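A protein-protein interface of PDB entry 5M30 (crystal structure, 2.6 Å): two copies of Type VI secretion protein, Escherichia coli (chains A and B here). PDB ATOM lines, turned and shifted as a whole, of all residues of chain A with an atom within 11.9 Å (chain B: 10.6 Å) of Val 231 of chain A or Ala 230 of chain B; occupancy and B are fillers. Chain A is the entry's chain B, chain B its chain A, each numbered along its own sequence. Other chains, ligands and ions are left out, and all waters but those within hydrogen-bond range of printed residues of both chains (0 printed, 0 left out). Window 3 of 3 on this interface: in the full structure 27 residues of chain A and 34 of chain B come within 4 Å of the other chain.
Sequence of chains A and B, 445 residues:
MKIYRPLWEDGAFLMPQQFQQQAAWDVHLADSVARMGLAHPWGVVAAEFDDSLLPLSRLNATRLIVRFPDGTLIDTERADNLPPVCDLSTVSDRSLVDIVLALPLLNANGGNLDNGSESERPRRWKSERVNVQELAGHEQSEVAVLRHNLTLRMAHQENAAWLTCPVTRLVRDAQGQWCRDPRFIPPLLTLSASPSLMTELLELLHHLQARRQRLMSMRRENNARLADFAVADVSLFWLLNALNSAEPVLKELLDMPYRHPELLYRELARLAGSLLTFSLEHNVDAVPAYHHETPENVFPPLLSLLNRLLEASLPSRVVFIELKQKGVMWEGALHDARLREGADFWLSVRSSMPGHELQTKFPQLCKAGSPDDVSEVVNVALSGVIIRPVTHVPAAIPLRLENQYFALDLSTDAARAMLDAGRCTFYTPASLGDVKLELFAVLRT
Among the printed residues, merely in contact across the chains: Ala 232 of chain A with Phe 229 of chain B (3.2 Å), Phe 278 of chain A with Phe 237 of chain B (3.3 Å), Ser 235 of chain A with Phe 229 of chain B (3.4 Å), Trp 238 of chain A with Trp 238 of chain B (3.4 Å), Val 234 of chain A with Phe 229 of chain B (3.7 Å), Val 234 of chain A with Phe 237 of chain B (3.7 Å), Val 231 of chain A with Val 234 of chain B (3.7 Å), Val 231 of chain A with Phe 229 of chain B (3.7 Å), Trp 238 of chain A with Phe 237 of chain B (3.8 Å), Val 234 of chain A with Val 234 of chain B (3.8 Å) and Val 231 of chain A with Ala 230 of chain B (3.97 Å).
Val 231 of chain A touches three residues of chain B. Of chain A, only Val 231 comes within 4 Å of Ala 230 of chain B. Ala 230 of chain A touches none of the printed residues of chain B. Of chain B, only Phe 229 (3.2 Å) comes within 4 Å of Ala 232 of chain A. Asp 228 of chain B touches none of the printed residues of chain A. Of chain A, only Val 231 (3.7 Å), Ala 232 (3.2 Å), Val 234 (3.7 Å) and Ser 235 (3.4 Å) come within 4 Å of Phe 229 of chain B. Ala 232 of chain B touches none of the printed residues of chain A. No residue of chain A comes within 4 Å of Asp 233 of chain B. Val 234 of chain B touches just these residues of chain A: Val 231 and Val 234. Printed residues of chain A within 4 Å of Trp 238 of chain B: Trp 238 (3.4 Å). Printed residues of chain B within 4 Å of Val 234 of chain A: Phe 229 (3.7 Å), Val 234 (3.8 Å) and Phe 237 (3.7 Å). The nearest residue of chain B that does not touch Val 231 of chain A is Val 231 of chain B (4.4 Å). The nearest residue of chain A that does not touch Ala 230 of chain B is Val 234 of chain A (5.1 Å).
Of the 17 printed residues of chain A, 6 touch a printed residue of chain B. Hydrophobic or aromatic side chains of chain A within 4 Å of the printed part of chain B: Val 231, Val 234, Trp 238 and Phe 278. Along chain A the printed residues that touch a printed residue of chain B span positions 231 to 278. Along chain B the printed residues that touch a printed residue of chain A span positions 229 to 238.
Val 231 of chain A touches Val 234 of chain B, but with the chains exchanged Val 234 of chain A does not touch Val 231 of chain B (6.9 Å). Val 234 of chain A touches Phe 229 of chain B, but with the chains exchanged Phe 229 of chain A does not touch Val 234 of chain B (8.4 Å). Trp 238 of chain A touches Phe 237 of chain B, but with the chains exchanged Phe 237 of chain A does not touch Trp 238 of chain B (7.1 Å). Trp 238 of chain B touches its own counterpart, Trp 238 of chain A. 14 positions are printed for both chains. Of the 11 pairs that touch across the chains among the printed residues, 2 have their exchanged pair printed and touching as well.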
ATOM      1  N   ARG A 220     -28.121  -8.448   8.168  1.00  0.00           N
ATOM      2  CA  ARG A 220     -27.826  -9.216   6.933  1.00  0.00           C
ATOM      3  C   ARG A 220     -27.767 -10.752   7.144  1.00  0.00           C
ATOM      4  O   ARG A 220     -26.780 -11.287   7.672  1.00  0.00           O
ATOM      5  CB  ARG A 220     -26.545  -8.703   6.232  1.00  0.00           C
ATOM      6  CG  ARG A 220     -26.779  -7.575   5.235  1.00  0.00           C
ATOM      7  CD  ARG A 220     -25.488  -7.159   4.559  1.00  0.00           C
ATOM      8  N   ALA A 227     -25.875 -13.218  10.591  1.00  0.00           N
ATOM      9  CA  ALA A 227     -24.486 -13.546  10.880  1.00  0.00           C
ATOM     10  C   ALA A 227     -23.477 -12.775  10.001  1.00  0.00           C
ATOM     11  O   ALA A 227     -22.336 -12.576  10.434  1.00  0.00           O
ATOM     12  CB  ALA A 227     -24.272 -15.047  10.757  1.00  0.00           C
ATOM     13  N   ASP A 228     -23.897 -12.327   8.794  1.00  0.00           N
ATOM     14  CA  ASP A 228     -23.046 -11.616   7.830  1.00  0.00           C
ATOM     15  C   ASP A 228     -22.736 -10.164   8.204  1.00  0.00           C
ATOM     16  O   ASP A 228     -23.648  -9.343   8.348  1.00  0.00           O
ATOM     17  CB  ASP A 228     -23.629 -11.690   6.410  1.00  0.00           C
ATOM     18  N   PHE A 229     -21.429  -9.858   8.338  1.00  0.00           N
ATOM     19  CA  PHE A 229     -20.891  -8.529   8.647  1.00  0.00           C
ATOM     20  C   PHE A 229     -19.778  -8.186   7.648  1.00  0.00           C
ATOM     21  O   PHE A 229     -18.958  -9.051   7.317  1.00  0.00           O
ATOM     22  CB  PHE A 229     -20.370  -8.458  10.095  1.00  0.00           C
ATOM     23  N   ALA A 230     -19.776  -6.931   7.145  1.00  0.00           N
ATOM     24  CA  ALA A 230     -18.810  -6.416   6.164  1.00  0.00           C
ATOM     25  C   ALA A 230     -18.461  -4.939   6.435  1.00  0.00           C
ATOM     26  O   ALA A 230     -19.062  -4.335   7.324  1.00  0.00           O
ATOM     27  CB  ALA A 230     -19.358  -6.589   4.752  1.00  0.00           C
ATOM     28  N   VAL A 231     -17.500  -4.363   5.669  1.00  0.00           N
ATOM     29  CA  VAL A 231     -17.016  -2.974   5.788  1.00  0.00           C
ATOM     30  C   VAL A 231     -18.097  -1.881   5.623  1.00  0.00           C
ATOM     31  O   VAL A 231     -17.916  -0.759   6.108  1.00  0.00           O
ATOM     32  CB  VAL A 231     -15.844  -2.716   4.818  1.00  0.00           C
ATOM     33  N   ALA A 232     -19.206  -2.212   4.938  1.00  0.00           N
ATOM     34  CA  ALA A 232     -20.324  -1.309   4.652  1.00  0.00           C
ATOM     35  C   ALA A 232     -21.151  -0.865   5.881  1.00  0.00           C
ATOM     36  O   ALA A 232     -21.501   0.315   5.969  1.00  0.00           O
ATOM     37  CB  ALA A 232     -21.239  -1.925   3.599  1.00  0.00           C
ATOM     38  N   ASP A 233     -21.491  -1.798   6.804  1.00  0.00           N
ATOM     39  CA  ASP A 233     -22.323  -1.470   7.967  1.00  0.00           C
ATOM     40  C   ASP A 233     -21.592  -1.608   9.328  1.00  0.00           C
ATOM     41  O   ASP A 233     -21.803  -2.573  10.074  1.00  0.00           O
ATOM     42  CB  ASP A 233     -23.659  -2.256   7.950  1.00  0.00           C
ATOM     43  CG  ASP A 233     -23.576  -3.737   7.592  1.00  0.00           C
ATOM     44  OD1 ASP A 233     -22.495  -4.341   7.787  1.00  0.00           O
ATOM     45  OD2 ASP A 233     -24.602  -4.297   7.139  1.00  0.00           O
ATOM     46  N   VAL A 234     -20.745  -0.599   9.649  1.00  0.00           N
ATOM     47  CA  VAL A 234     -20.042  -0.507  10.935  1.00  0.00           C
ATOM     48  C   VAL A 234     -21.054  -0.002  11.986  1.00  0.00           C
ATOM     49  O   VAL A 234     -20.971  -0.397  13.149  1.00  0.00           O
ATOM     50  CB  VAL A 234     -18.691   0.293  10.921  1.00  0.00           C
ATOM     51  CG1 VAL A 234     -17.802  -0.109   9.752  1.00  0.00           C
ATOM     52  CG2 VAL A 234     -18.893   1.807  10.955  1.00  0.00           C
ATOM     53  N   SER A 235     -22.031   0.841  11.540  1.00  0.00           N
ATOM     54  CA  SER A 235     -23.114   1.425  12.342  1.00  0.00           C
ATOM     55  C   SER A 235     -24.058   0.346  12.843  1.00  0.00           C
ATOM     56  O   SER A 235     -24.378   0.354  14.020  1.00  0.00           O
ATOM     57  CB  SER A 235     -23.891   2.478  11.551  1.00  0.00           C
ATOM     58  OG  SER A 235     -24.395   1.953  10.333  1.00  0.00           O
ATOM     59  N   LEU A 236     -24.473  -0.598  11.975  1.00  0.00           N
ATOM     60  CA  LEU A 236     -25.353  -1.682  12.401  1.00  0.00           C
ATOM     61  C   LEU A 236     -24.667  -2.609  13.399  1.00  0.00           C
ATOM     62  O   LEU A 236     -25.324  -3.063  14.335  1.00  0.00           O
ATOM     63  CB  LEU A 236     -25.912  -2.473  11.205  1.00  0.00           C
ATOM     64  CG  LEU A 236     -27.249  -3.231  11.389  1.00  0.00           C
ATOM     65  CD1 LEU A 236     -27.036  -4.696  11.710  1.00  0.00           C
ATOM     66  CD2 LEU A 236     -28.196  -2.537  12.366  1.00  0.00           C
ATOM     67  N   PHE A 237     -23.353  -2.866  13.225  1.00  0.00           N
ATOM     68  CA  PHE A 237     -22.631  -3.726  14.154  1.00  0.00           C
ATOM     69  C   PHE A 237     -22.378  -3.064  15.492  1.00  0.00           C
ATOM     70  O   PHE A 237     -22.766  -3.633  16.514  1.00  0.00           O
ATOM     71  CB  PHE A 237     -21.306  -4.288  13.591  1.00  0.00           C
ATOM     72  CG  PHE A 237     -20.464  -4.937  14.678  1.00  0.00           C
ATOM     73  CD1 PHE A 237     -20.824  -6.169  15.219  1.00  0.00           C
ATOM     74  CD2 PHE A 237     -19.363  -4.280  15.217  1.00  0.00           C
ATOM     75  CE1 PHE A 237     -20.078  -6.742  16.259  1.00  0.00           C
ATOM     76  CE2 PHE A 237     -18.621  -4.856  16.253  1.00  0.00           C
ATOM     77  CZ  PHE A 237     -18.981  -6.085  16.763  1.00  0.00           C
ATOM     78  N   TRP A 238     -21.651  -1.918  15.497  1.00  0.00           N
ATOM     79  CA  TRP A 238     -21.260  -1.241  16.730  1.00  0.00           C
ATOM     80  C   TRP A 238     -22.456  -0.733  17.525  1.00  0.00           C
ATOM     81  O   TRP A 238     -22.353  -0.702  18.746  1.00  0.00           O
ATOM     82  CB  TRP A 238     -20.201  -0.153  16.502  1.00  0.00           C
ATOM     83  CG  TRP A 238     -18.859  -0.667  16.059  1.00  0.00           C
ATOM     84  CD1 TRP A 238     -18.276  -0.498  14.834  1.00  0.00           C
ATOM     85  CD2 TRP A 238     -17.944  -1.461  16.833  1.00  0.00           C
ATOM     86  NE1 TRP A 238     -17.051  -1.125  14.801  1.00  0.00           N
ATOM     87  CE2 TRP A 238     -16.828  -1.738  16.010  1.00  0.00           C
ATOM     88  CE3 TRP A 238     -17.959  -1.972  18.147  1.00  0.00           C
ATOM     89  CZ2 TRP A 238     -15.740  -2.499  16.458  1.00  0.00           C
ATOM     90  CZ3 TRP A 238     -16.879  -2.722  18.588  1.00  0.00           C
ATOM     91  CH2 TRP A 238     -15.780  -2.965  17.755  1.00  0.00           C
ATOM     92  N   PHE A 278     -21.445   7.325  16.880  1.00  0.00           N
ATOM     93  CA  PHE A 278     -22.211   7.597  15.668  1.00  0.00           C
ATOM     94  C   PHE A 278     -23.085   8.846  15.783  1.00  0.00           C
ATOM     95  O   PHE A 278     -24.155   8.882  15.180  1.00  0.00           O
ATOM     96  CB  PHE A 278     -23.068   6.390  15.276  1.00  0.00           C
ATOM     97  CG  PHE A 278     -22.382   5.073  15.480  1.00  0.00           C
ATOM     98  CD1 PHE A 278     -21.413   4.626  14.580  1.00  0.00           C
ATOM     99  CD2 PHE A 278     -22.673   4.284  16.589  1.00  0.00           C
ATOM    100  CE1 PHE A 278     -20.757   3.406  14.784  1.00  0.00           C
ATOM    101  CE2 PHE A 278     -22.019   3.063  16.789  1.00  0.00           C
ATOM    102  CZ  PHE A 278     -21.049   2.646  15.895  1.00  0.00           C
ATOM    103  N   PRO A 315     -29.371   3.440  11.020  1.00  0.00           N
ATOM    104  CA  PRO A 315     -28.353   3.416   9.940  1.00  0.00           C
ATOM    105  C   PRO A 315     -28.958   3.654   8.535  1.00  0.00           C
ATOM    106  O   PRO A 315     -30.188   3.628   8.390  1.00  0.00           O
ATOM    107  CB  PRO A 315     -27.729   2.012  10.061  1.00  0.00           C
ATOM    108  CG  PRO A 315     -28.217   1.453  11.364  1.00  0.00           C
ATOM    109  CD  PRO A 315     -29.539   2.099  11.617  1.00  0.00           C
ATOM    110  N   SER A 316     -28.102   3.904   7.505  1.00  0.00           N
ATOM    111  CA  SER A 316     -28.545   4.165   6.124  1.00  0.00           C
ATOM    112  C   SER A 316     -29.384   3.017   5.543  1.00  0.00           C
ATOM    113  O   SER A 316     -28.863   1.932   5.251  1.00  0.00           O
ATOM    114  CB  SER A 316     -27.369   4.513   5.214  1.00  0.00           C
ATOM    115  OG  SER A 316     -26.492   3.412   5.036  1.00  0.00           O
ATOM    116  N   ARG A 338     -30.679  -7.612   1.187  1.00  0.00           N
ATOM    117  CA  ARG A 338     -31.562  -6.739   1.975  1.00  0.00           C
ATOM    118  C   ARG A 338     -32.867  -6.353   1.259  1.00  0.00           C
ATOM    119  O   ARG A 338     -33.861  -6.062   1.933  1.00  0.00           O
ATOM    120  CB  ARG A 338     -30.814  -5.487   2.461  1.00  0.00           C
ATOM    121  CG  ARG A 338     -29.741  -5.770   3.518  1.00  0.00           C
ATOM    122  CD  ARG A 338     -28.875  -4.552   3.796  1.00  0.00           C
ATOM    123  NE  ARG A 338     -28.107  -4.145   2.616  1.00  0.00           N
ATOM    124  CZ  ARG A 338     -27.859  -2.884   2.273  1.00  0.00           C
ATOM    125  NH1 ARG A 338     -28.312  -1.882   3.021  1.00  0.00           N
ATOM    126  NH2 ARG A 338     -27.163  -2.613   1.179  1.00  0.00           N
ATOM    127  N   MET B 218     -11.777  13.121  12.758  1.00  0.00           N
ATOM    128  CA  MET B 218     -11.388  12.288  11.613  1.00  0.00           C
ATOM    129  C   MET B 218     -12.539  11.423  11.004  1.00  0.00           C
ATOM    130  O   MET B 218     -12.259  10.571  10.156  1.00  0.00           O
ATOM    131  CB  MET B 218     -10.168  11.414  11.965  1.00  0.00           C
ATOM    132  N   ARG B 219     -13.815  11.656  11.397  1.00  0.00           N
ATOM    133  CA  ARG B 219     -14.986  10.950  10.829  1.00  0.00           C
ATOM    134  C   ARG B 219     -15.827  11.902   9.986  1.00  0.00           C
ATOM    135  O   ARG B 219     -16.077  13.049  10.395  1.00  0.00           O
ATOM    136  CB  ARG B 219     -15.869  10.162  11.845  1.00  0.00           C
ATOM    137  CG  ARG B 219     -15.701  10.454  13.337  1.00  0.00           C
ATOM    138  CD  ARG B 219     -17.021  10.414  14.107  1.00  0.00           C
ATOM    139  NE  ARG B 219     -17.248  11.678  14.813  1.00  0.00           N
ATOM    140  CZ  ARG B 219     -18.332  11.981  15.514  1.00  0.00           C
ATOM    141  NH1 ARG B 219     -19.326  11.108  15.623  1.00  0.00           N
ATOM    142  NH2 ARG B 219     -18.427  13.156  16.126  1.00  0.00           N
ATOM    143  N   ARG B 220     -16.250  11.416   8.799  1.00  0.00           N
ATOM    144  CA  ARG B 220     -17.018  12.180   7.813  1.00  0.00           C
ATOM    145  C   ARG B 220     -18.309  11.498   7.394  1.00  0.00           C
ATOM    146  O   ARG B 220     -19.315  12.174   7.187  1.00  0.00           O
ATOM    147  CB  ARG B 220     -16.153  12.541   6.583  1.00  0.00           C
ATOM    148  CG  ARG B 220     -14.990  11.581   6.270  1.00  0.00           C
ATOM    149  CD  ARG B 220     -15.323  10.567   5.187  1.00  0.00           C
ATOM    150  NE  ARG B 220     -14.378   9.448   5.179  1.00  0.00           N
ATOM    151  CZ  ARG B 220     -14.685   8.206   4.818  1.00  0.00           C
ATOM    152  NH1 ARG B 220     -13.763   7.253   4.846  1.00  0.00           N
ATOM    153  NH2 ARG B 220     -15.921   7.904   4.431  1.00  0.00           N
ATOM    154  N   ALA B 227     -22.985   9.936   7.152  1.00  0.00           N
ATOM    155  CA  ALA B 227     -21.699   9.325   6.789  1.00  0.00           C
ATOM    156  C   ALA B 227     -21.826   7.993   6.036  1.00  0.00           C
ATOM    157  O   ALA B 227     -22.725   7.198   6.327  1.00  0.00           O
ATOM    158  CB  ALA B 227     -20.839   9.136   8.029  1.00  0.00           C
ATOM    159  N   ASP B 228     -20.906   7.756   5.077  1.00  0.00           N
ATOM    160  CA  ASP B 228     -20.789   6.526   4.279  1.00  0.00           C
ATOM    161  C   ASP B 228     -19.435   5.906   4.637  1.00  0.00           C
ATOM    162  O   ASP B 228     -18.414   6.596   4.564  1.00  0.00           O
ATOM    163  CB  ASP B 228     -20.888   6.828   2.777  1.00  0.00           C
ATOM    164  N   PHE B 229     -19.428   4.633   5.069  1.00  0.00           N
ATOM    165  CA  PHE B 229     -18.218   3.962   5.571  1.00  0.00           C
ATOM    166  C   PHE B 229     -17.289   3.374   4.506  1.00  0.00           C
ATOM    167  O   PHE B 229     -17.692   3.119   3.372  1.00  0.00           O
ATOM    168  CB  PHE B 229     -18.561   2.893   6.628  1.00  0.00           C
ATOM    169  CG  PHE B 229     -19.523   3.376   7.685  1.00  0.00           C
ATOM    170  CD1 PHE B 229     -20.713   2.706   7.920  1.00  0.00           C
ATOM    171  CD2 PHE B 229     -19.273   4.545   8.396  1.00  0.00           C
ATOM    172  CE1 PHE B 229     -21.622   3.177   8.867  1.00  0.00           C
ATOM    173  CE2 PHE B 229     -20.187   5.019   9.335  1.00  0.00           C
ATOM    174  CZ  PHE B 229     -21.352   4.329   9.568  1.00  0.00           C
ATOM    175  N   ALA B 230     -16.025   3.175   4.919  1.00  0.00           N
ATOM    176  CA  ALA B 230     -14.907   2.644   4.141  1.00  0.00           C
ATOM    177  C   ALA B 230     -14.142   1.590   4.964  1.00  0.00           C
ATOM    178  O   ALA B 230     -14.528   1.310   6.102  1.00  0.00           O
ATOM    179  CB  ALA B 230     -13.972   3.789   3.761  1.00  0.00           C
ATOM    180  N   VAL B 231     -13.066   1.008   4.383  1.00  0.00           N
ATOM    181  CA  VAL B 231     -12.183   0.016   5.017  1.00  0.00           C
ATOM    182  C   VAL B 231     -11.451   0.677   6.208  1.00  0.00           C
ATOM    183  O   VAL B 231     -11.350   0.078   7.284  1.00  0.00           O
ATOM    184  CB  VAL B 231     -11.211  -0.621   3.973  1.00  0.00           C
ATOM    185  CG1 VAL B 231      -9.986  -1.262   4.625  1.00  0.00           C
ATOM    186  CG2 VAL B 231     -11.938  -1.637   3.093  1.00  0.00           C
ATOM    187  N   ALA B 232     -10.983   1.933   6.006  1.00  0.00           N
ATOM    188  CA  ALA B 232     -10.291   2.771   6.994  1.00  0.00           C
ATOM    189  C   ALA B 232     -11.192   3.083   8.192  1.00  0.00           C
ATOM    190  O   ALA B 232     -10.692   3.170   9.317  1.00  0.00           O
ATOM    191  CB  ALA B 232      -9.820   4.067   6.345  1.00  0.00           C
ATOM    192  N   ASP B 233     -12.517   3.235   7.945  1.00  0.00           N
ATOM    193  CA  ASP B 233     -13.540   3.498   8.962  1.00  0.00           C
ATOM    194  C   ASP B 233     -13.744   2.321   9.927  1.00  0.00           C
ATOM    195  O   ASP B 233     -13.932   2.553  11.113  1.00  0.00           O
ATOM    196  CB  ASP B 233     -14.870   3.933   8.313  1.00  0.00           C
ATOM    197  CG  ASP B 233     -14.980   5.422   7.999  1.00  0.00           C
ATOM    198  OD1 ASP B 233     -13.926   6.091   7.883  1.00  0.00           O
ATOM    199  OD2 ASP B 233     -16.116   5.911   7.838  1.00  0.00           O
ATOM    200  N   VAL B 234     -13.667   1.072   9.429  1.00  0.00           N
ATOM    201  CA  VAL B 234     -13.797  -0.168  10.212  1.00  0.00           C
ATOM    202  C   VAL B 234     -12.906  -0.107  11.472  1.00  0.00           C
ATOM    203  O   VAL B 234     -13.414  -0.237  12.585  1.00  0.00           O
ATOM    204  CB  VAL B 234     -13.510  -1.424   9.332  1.00  0.00           C
ATOM    205  CG1 VAL B 234     -13.309  -2.681  10.173  1.00  0.00           C
ATOM    206  CG2 VAL B 234     -14.619  -1.634   8.311  1.00  0.00           C
ATOM    207  N   SER B 235     -11.596   0.141  11.280  1.00  0.00           N
ATOM    208  CA  SER B 235     -10.605   0.289  12.345  1.00  0.00           C
ATOM    209  C   SER B 235     -10.909   1.523  13.204  1.00  0.00           C
ATOM    210  O   SER B 235     -10.875   1.424  14.423  1.00  0.00           O
ATOM    211  CB  SER B 235      -9.198   0.381  11.765  1.00  0.00           C
ATOM    212  OG  SER B 235      -9.048   1.528  10.943  1.00  0.00           O
ATOM    213  N   LEU B 236     -11.220   2.669  12.573  1.00  0.00           N
ATOM    214  CA  LEU B 236     -11.544   3.918  13.259  1.00  0.00           C
ATOM    215  C   LEU B 236     -12.732   3.768  14.237  1.00  0.00           C
ATOM    216  O   LEU B 236     -12.637   4.204  15.379  1.00  0.00           O
ATOM    217  CB  LEU B 236     -11.807   5.032  12.221  1.00  0.00           C
ATOM    218  CG  LEU B 236     -12.542   6.306  12.674  1.00  0.00           C
ATOM    219  CD1 LEU B 236     -11.588   7.323  13.251  1.00  0.00           C
ATOM    220  CD2 LEU B 236     -13.296   6.919  11.522  1.00  0.00           C
ATOM    221  N   PHE B 237     -13.826   3.140  13.792  1.00  0.00           N
ATOM    222  CA  PHE B 237     -15.034   2.935  14.585  1.00  0.00           C
ATOM    223  C   PHE B 237     -14.856   1.851  15.675  1.00  0.00           C
ATOM    224  O   PHE B 237     -15.614   1.839  16.643  1.00  0.00           O
ATOM    225  CB  PHE B 237     -16.253   2.691  13.674  1.00  0.00           C
ATOM    226  CG  PHE B 237     -16.815   3.986  13.115  1.00  0.00           C
ATOM    227  CD1 PHE B 237     -16.257   4.582  11.988  1.00  0.00           C
ATOM    228  CD2 PHE B 237     -17.881   4.625  13.734  1.00  0.00           C
ATOM    229  CE1 PHE B 237     -16.764   5.788  11.489  1.00  0.00           C
ATOM    230  CE2 PHE B 237     -18.388   5.830  13.234  1.00  0.00           C
ATOM    231  CZ  PHE B 237     -17.822   6.406  12.122  1.00  0.00           C
ATOM    232  N   TRP B 238     -13.811   1.013  15.567  1.00  0.00           N
ATOM    233  CA  TRP B 238     -13.446   0.025  16.588  1.00  0.00           C
ATOM    234  C   TRP B 238     -12.778   0.780  17.739  1.00  0.00           C
ATOM    235  O   TRP B 238     -13.112   0.581  18.912  1.00  0.00           O
ATOM    236  CB  TRP B 238     -12.486  -1.032  15.995  1.00  0.00           C
ATOM    237  CG  TRP B 238     -11.469  -1.604  16.952  1.00  0.00           C
ATOM    238  CD1 TRP B 238     -11.674  -2.593  17.870  1.00  0.00           C
ATOM    239  CD2 TRP B 238     -10.077  -1.245  17.054  1.00  0.00           C
ATOM    240  NE1 TRP B 238     -10.504  -2.868  18.544  1.00  0.00           N
ATOM    241  CE2 TRP B 238      -9.507  -2.056  18.062  1.00  0.00           C
ATOM    242  CE3 TRP B 238      -9.261  -0.296  16.411  1.00  0.00           C
ATOM    243  CZ2 TRP B 238      -8.153  -1.961  18.427  1.00  0.00           C
ATOM    244  CZ3 TRP B 238      -7.928  -0.189  16.788  1.00  0.00           C
ATOM    245  CH2 TRP B 238      -7.384  -1.019  17.778  1.00  0.00           C
ATOM    246  N   PRO B 315      -3.819   6.584  10.843  1.00  0.00           N
ATOM    247  CA  PRO B 315      -4.967   6.646   9.921  1.00  0.00           C
ATOM    248  C   PRO B 315      -4.650   6.744   8.416  1.00  0.00           C
ATOM    249  O   PRO B 315      -5.530   7.150   7.648  1.00  0.00           O
ATOM    250  CB  PRO B 315      -5.717   7.891  10.417  1.00  0.00           C
ATOM    251  CG  PRO B 315      -4.636   8.770  11.046  1.00  0.00           C
ATOM    252  CD  PRO B 315      -3.376   7.947  11.204  1.00  0.00           C
